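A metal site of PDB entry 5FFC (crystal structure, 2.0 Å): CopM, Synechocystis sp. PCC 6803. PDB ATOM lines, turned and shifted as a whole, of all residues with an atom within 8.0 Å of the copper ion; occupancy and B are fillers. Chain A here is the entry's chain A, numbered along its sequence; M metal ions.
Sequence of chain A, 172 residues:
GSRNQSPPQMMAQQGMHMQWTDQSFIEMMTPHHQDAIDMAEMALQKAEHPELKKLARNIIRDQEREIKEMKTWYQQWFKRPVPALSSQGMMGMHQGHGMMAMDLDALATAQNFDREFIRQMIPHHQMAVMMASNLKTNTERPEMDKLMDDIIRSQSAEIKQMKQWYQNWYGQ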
ATOM      1  N   MET A  28     -17.932  14.028  -0.664  1.00  0.00           N
ATOM      2  CA  MET A  28     -19.322  14.225  -1.023  1.00  0.00           C
ATOM      3  C   MET A  28     -19.552  14.082  -2.531  1.00  0.00           C
ATOM      4  O   MET A  28     -20.568  13.535  -2.962  1.00  0.00           O
ATOM      5  CB  MET A  28     -19.800  15.604  -0.560  1.00  0.00           C
ATOM      6  N   MET A  29     -18.602  14.584  -3.312  1.00  0.00           N
ATOM      7  CA  MET A  29     -18.767  14.623  -4.768  1.00  0.00           C
ATOM      8  C   MET A  29     -18.672  13.280  -5.460  1.00  0.00           C
ATOM      9  O   MET A  29     -19.339  13.045  -6.464  1.00  0.00           O
ATOM     10  CB  MET A  29     -17.819  15.629  -5.395  1.00  0.00           C
ATOM     11  CG  MET A  29     -18.326  17.049  -5.257  1.00  0.00           C
ATOM     12  SD  MET A  29     -19.993  17.202  -5.954  1.00  0.00           S
ATOM     13  CE  MET A  29     -19.640  16.900  -7.674  1.00  0.00           C
ATOM     14  N   THR A  30     -17.836  12.396  -4.917  1.00  0.00           N
ATOM     15  CA  THR A  30     -17.703  11.046  -5.465  1.00  0.00           C
ATOM     16  C   THR A  30     -19.039  10.280  -5.507  1.00  0.00           C
ATOM     17  O   THR A  30     -19.418   9.791  -6.573  1.00  0.00           O
ATOM     18  CB  THR A  30     -16.587  10.248  -4.741  1.00  0.00           C
ATOM     19  OG1 THR A  30     -15.382  11.026  -4.703  1.00  0.00           O
ATOM     20  CG2 THR A  30     -16.325   8.929  -5.467  1.00  0.00           C
ATOM     21  N   PRO A  31     -19.752  10.176  -4.371  1.00  0.00           N
ATOM     22  CA  PRO A  31     -21.067   9.526  -4.447  1.00  0.00           C
ATOM     23  C   PRO A  31     -22.041  10.284  -5.341  1.00  0.00           C
ATOM     24  O   PRO A  31     -22.860   9.662  -6.016  1.00  0.00           O
ATOM     25  CB  PRO A  31     -21.573   9.569  -2.996  1.00  0.00           C
ATOM     26  CG  PRO A  31     -20.349   9.747  -2.163  1.00  0.00           C
ATOM     27  CD  PRO A  31     -19.442  10.592  -2.992  1.00  0.00           C
ATOM     28  N   HIS A  32     -21.959  11.616  -5.327  1.00  0.00           N
ATOM     29  CA  HIS A  32     -22.840  12.436  -6.153  1.00  0.00           C
ATOM     30  C   HIS A  32     -22.620  12.230  -7.655  1.00  0.00           C
ATOM     31  O   HIS A  32     -23.565  12.275  -8.435  1.00  0.00           O
ATOM     32  CB  HIS A  32     -22.710  13.915  -5.801  1.00  0.00           C
ATOM     33  CG  HIS A  32     -23.798  14.414  -4.911  1.00  0.00           C
ATOM     34  ND1 HIS A  32     -25.129  14.146  -5.154  1.00  0.00           N
ATOM     35  CD2 HIS A  32     -23.766  15.177  -3.789  1.00  0.00           C
ATOM     36  CE1 HIS A  32     -25.868  14.708  -4.218  1.00  0.00           C
ATOM     37  NE2 HIS A  32     -25.066  15.348  -3.376  1.00  0.00           N
ATOM     38  N   HIS A  33     -21.371  12.034  -8.060  1.00  0.00           N
ATOM     39  CA  HIS A  33     -21.064  11.769  -9.466  1.00  0.00           C
ATOM     40  C   HIS A  33     -21.616  10.409  -9.873  1.00  0.00           C
ATOM     41  O   HIS A  33     -21.862  10.170 -11.054  1.00  0.00           O
ATOM     42  CB  HIS A  33     -19.557  11.840  -9.742  1.00  0.00           C
ATOM     43  CG  HIS A  33     -19.084  13.180 -10.240  1.00  0.00           C
ATOM     44  ND1 HIS A  33     -19.753  14.360  -9.964  1.00  0.00           N
ATOM     45  CD2 HIS A  33     -18.016  13.516 -10.989  1.00  0.00           C
ATOM     46  CE1 HIS A  33     -19.113  15.365 -10.529  1.00  0.00           C
ATOM     47  NE2 HIS A  33     -18.046  14.885 -11.156  1.00  0.00           N
ATOM     48  N   GLN A  34     -21.825   9.526  -8.909  1.00  0.00           N
ATOM     49  CA  GLN A  34     -22.293   8.177  -9.210  1.00  0.00           C
ATOM     50  C   GLN A  34     -23.748   8.123  -9.645  1.00  0.00           C
ATOM     51  O   GLN A  34     -24.066   7.480 -10.650  1.00  0.00           O
ATOM     52  CB  GLN A  34     -22.077   7.239  -8.021  1.00  0.00           C
ATOM     53  CG  GLN A  34     -22.463   5.783  -8.318  1.00  0.00           C
ATOM     54  CD  GLN A  34     -21.712   5.217  -9.505  1.00  0.00           C
ATOM     55  OE1 GLN A  34     -22.303   4.615 -10.398  1.00  0.00           O
ATOM     56  NE2 GLN A  34     -20.394   5.404  -9.519  1.00  0.00           N
ATOM     57  N   ASP A  35     -24.627   8.770  -8.893  1.00  0.00           N
ATOM     58  CA  ASP A  35     -26.050   8.755  -9.221  1.00  0.00           C
ATOM     59  C   ASP A  35     -26.295   9.349 -10.616  1.00  0.00           C
ATOM     60  O   ASP A  35     -27.161   8.884 -11.356  1.00  0.00           O
ATOM     61  CB  ASP A  35     -26.889   9.457  -8.142  1.00  0.00           C
ATOM     62  CG  ASP A  35     -26.460  10.903  -7.908  1.00  0.00           C
ATOM     63  OD1 ASP A  35     -26.128  11.597  -8.881  1.00  0.00           O
ATOM     64  OD2 ASP A  35     -26.483  11.352  -6.741  1.00  0.00           O
ATOM     65  N   ALA A  36     -25.520  10.376 -10.953  1.00  0.00           N
ATOM     66  CA  ALA A  36     -25.597  10.985 -12.275  1.00  0.00           C
ATOM     67  C   ALA A  36     -25.250   9.972 -13.362  1.00  0.00           C
ATOM     68  O   ALA A  36     -25.966   9.848 -14.348  1.00  0.00           O
ATOM     69  CB  ALA A  36     -24.660  12.171 -12.358  1.00  0.00           C
ATOM     70  N   ILE A  37     -24.155   9.250 -13.142  1.00  0.00           N
ATOM     71  CA  ILE A  37     -23.706   8.222 -14.072  1.00  0.00           C
ATOM     72  C   ILE A  37     -24.797   7.170 -14.288  1.00  0.00           C
ATOM     73  O   ILE A  37     -25.070   6.791 -15.422  1.00  0.00           O
ATOM     74  CB  ILE A  37     -22.383   7.572 -13.610  1.00  0.00           C
ATOM     75  CG1 ILE A  37     -21.229   8.554 -13.783  1.00  0.00           C
ATOM     76  CG2 ILE A  37     -22.098   6.291 -14.396  1.00  0.00           C
ATOM     77  CD1 ILE A  37     -19.898   8.053 -13.267  1.00  0.00           C
ATOM     78  N   GLN A  63     -17.759  12.474 -15.977  1.00  0.00           N
ATOM     79  CA  GLN A  63     -17.897  12.296 -14.550  1.00  0.00           C
ATOM     80  C   GLN A  63     -17.141  11.085 -14.031  1.00  0.00           C
ATOM     81  O   GLN A  63     -16.647  11.080 -12.909  1.00  0.00           O
ATOM     82  CB  GLN A  63     -19.375  12.353 -14.140  1.00  0.00           C
ATOM     83  CG  GLN A  63     -20.007  13.686 -14.540  1.00  0.00           C
ATOM     84  CD  GLN A  63     -21.175  14.085 -13.659  1.00  0.00           C
ATOM     85  OE1 GLN A  63     -21.342  13.571 -12.547  1.00  0.00           O
ATOM     86  NE2 GLN A  63     -22.004  15.012 -14.147  1.00  0.00           N
ATOM     87  N   MET A  93     -26.606   7.000  -0.556  1.00  0.00           N
ATOM     88  CA  MET A  93     -27.120   8.185  -1.251  1.00  0.00           C
ATOM     89  C   MET A  93     -28.537   7.970  -1.788  1.00  0.00           C
ATOM     90  O   MET A  93     -28.750   7.177  -2.690  1.00  0.00           O
ATOM     91  CB  MET A  93     -26.202   8.561  -2.413  1.00  0.00           C
ATOM     92  CG  MET A  93     -25.244   9.701  -2.105  1.00  0.00           C
ATOM     93  SD  MET A  93     -26.068  11.281  -1.881  1.00  0.00           S
ATOM     94  CE  MET A  93     -24.652  12.380  -1.960  1.00  0.00           C
ATOM     95  N   HIS A  94     -29.484   8.708  -1.221  1.00  0.00           N
ATOM     96  CA  HIS A  94     -30.887   8.596  -1.617  1.00  0.00           C
ATOM     97  C   HIS A  94     -31.703   9.747  -1.027  1.00  0.00           C
ATOM     98  O   HIS A  94     -31.261  10.423  -0.105  1.00  0.00           O
ATOM     99  CB  HIS A  94     -31.478   7.253  -1.195  1.00  0.00           C
ATOM    100  CG  HIS A  94     -31.273   6.922   0.250  1.00  0.00           C
ATOM    101  ND1 HIS A  94     -30.026   6.768   0.816  1.00  0.00           N
ATOM    102  CD2 HIS A  94     -32.161   6.708   1.251  1.00  0.00           C
ATOM    103  CE1 HIS A  94     -30.149   6.485   2.094  1.00  0.00           C
ATOM    104  NE2 HIS A  94     -31.436   6.432   2.381  1.00  0.00           N
ATOM    105  N   MET A  99     -29.658  15.484   0.818  1.00  0.00           N
ATOM    106  CA  MET A  99     -28.410  15.284   0.091  1.00  0.00           C
ATOM    107  C   MET A  99     -28.545  15.728  -1.371  1.00  0.00           C
ATOM    108  O   MET A  99     -27.568  15.749  -2.110  1.00  0.00           O
ATOM    109  CB  MET A  99     -27.959  13.825   0.151  1.00  0.00           C
ATOM    110  CG  MET A  99     -27.636  13.331   1.556  1.00  0.00           C
ATOM    111  SD  MET A  99     -26.158  14.094   2.253  1.00  0.00           S
ATOM    112  CE  MET A  99     -24.879  13.025   1.589  1.00  0.00           C
ATOM    113  N   MET A 100     -29.772  16.074  -1.762  1.00  0.00           N
ATOM    114  CA  MET A 100     -30.113  16.433  -3.137  1.00  0.00           C
ATOM    115  C   MET A 100     -29.827  15.276  -4.089  1.00  0.00           C
ATOM    116  O   MET A 100     -29.328  15.481  -5.193  1.00  0.00           O
ATOM    117  CB  MET A 100     -29.413  17.713  -3.585  1.00  0.00           C
ATOM    118  CG  MET A 100     -29.531  18.860  -2.591  1.00  0.00           C
ATOM    119  SD  MET A 100     -28.892  20.429  -3.214  1.00  0.00           S
ATOM    120  CE  MET A 100     -30.320  21.057  -4.094  1.00  0.00           C
ATOM    121  N   ALA A 101     -30.159  14.055  -3.660  1.00  0.00           N
ATOM    122  CA  ALA A 101     -29.960  12.875  -4.479  1.00  0.00           C
ATOM    123  C   ALA A 101     -31.092  12.730  -5.489  1.00  0.00           C
ATOM    124  O   ALA A 101     -32.102  13.429  -5.417  1.00  0.00           O
ATOM    125  CB  ALA A 101     -29.872  11.630  -3.607  1.00  0.00           C
ATOM    126  N   MET A 102     -30.926  11.803  -6.429  1.00  0.00           N
ATOM    127  CA  MET A 102     -31.913  11.586  -7.481  1.00  0.00           C
ATOM    128  C   MET A 102     -32.708  10.296  -7.269  1.00  0.00           C
ATOM    129  O   MET A 102     -32.425   9.509  -6.368  1.00  0.00           O
ATOM    130  CB  MET A 102     -31.240  11.641  -8.856  1.00  0.00           C
ATOM    131  CG  MET A 102     -30.691  13.035  -9.152  1.00  0.00           C
ATOM    132  SD  MET A 102     -30.059  13.280 -10.822  1.00  0.00           S
ATOM    133  CE  MET A 102     -28.571  12.284 -10.764  1.00  0.00           C
ATOM    134  N   HIS A 124     -29.543  18.700 -10.123  1.00  0.00           N
ATOM    135  CA  HIS A 124     -28.348  17.933  -9.757  1.00  0.00           C
ATOM    136  C   HIS A 124     -27.091  18.575 -10.334  1.00  0.00           C
ATOM    137  O   HIS A 124     -26.056  18.652  -9.653  1.00  0.00           O
ATOM    138  CB  HIS A 124     -28.470  16.486 -10.215  1.00  0.00           C
ATOM    139  CG  HIS A 124     -27.451  15.573  -9.616  1.00  0.00           C
ATOM    140  ND1 HIS A 124     -26.220  15.330 -10.183  1.00  0.00           N
ATOM    141  CD2 HIS A 124     -27.472  14.847  -8.469  1.00  0.00           C
ATOM    142  CE1 HIS A 124     -25.530  14.499  -9.432  1.00  0.00           C
ATOM    143  NE2 HIS A 124     -26.270  14.185  -8.383  1.00  0.00           N
ATOM    144  N   HIS A 125     -27.171  19.025 -11.588  1.00  0.00           N
ATOM    145  CA  HIS A 125     -26.057  19.754 -12.201  1.00  0.00           C
ATOM    146  C   HIS A 125     -25.802  21.096 -11.509  1.00  0.00           C
ATOM    147  O   HIS A 125     -24.652  21.465 -11.248  1.00  0.00           O
ATOM    148  CB  HIS A 125     -26.324  19.975 -13.698  1.00  0.00           C
ATOM    149  CG  HIS A 125     -25.729  18.932 -14.589  1.00  0.00           C
ATOM    150  ND1 HIS A 125     -25.730  17.590 -14.273  1.00  0.00           N
ATOM    151  CD2 HIS A 125     -25.134  19.033 -15.802  1.00  0.00           C
ATOM    152  CE1 HIS A 125     -25.146  16.914 -15.246  1.00  0.00           C
ATOM    153  NE2 HIS A 125     -24.767  17.760 -16.188  1.00  0.00           N
ATOM    154  N   MET A 127     -26.406  21.869  -8.464  1.00  0.00           N
ATOM    155  CA  MET A 127     -25.769  21.547  -7.196  1.00  0.00           C
ATOM    156  C   MET A 127     -24.249  21.389  -7.344  1.00  0.00           C
ATOM    157  O   MET A 127     -23.492  21.943  -6.546  1.00  0.00           O
ATOM    158  CB  MET A 127     -26.375  20.265  -6.617  1.00  0.00           C
ATOM    159  CG  MET A 127     -25.839  19.861  -5.256  1.00  0.00           C
ATOM    160  SD  MET A 127     -24.665  18.499  -5.371  1.00  0.00           S
ATOM    161  CE  MET A 127     -25.545  17.373  -6.448  1.00  0.00           C
HETATM  162 CU    CU M   1     -26.015  13.084  -6.485  1.00  0.00          CU
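The copper ion is bound by OD2 of Asp 35 (1.8 Å), ND1 of His 32 (1.9 Å) and NE2 of His 124 (2.2 Å). The copper ion has three donor atoms within binding distance. Slightly farther from the copper ion lies OD1 of Asp 35 (2.8 Å).
Of the 20 residues printed, 3 come within 4 Å of the copper ion.
NE2 of His 32 lies close to SD of Met 127, at 3.8 Å. O of Met 99 is in hydrogen-bond range of NE2 of His 32, 2.8 Å away.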
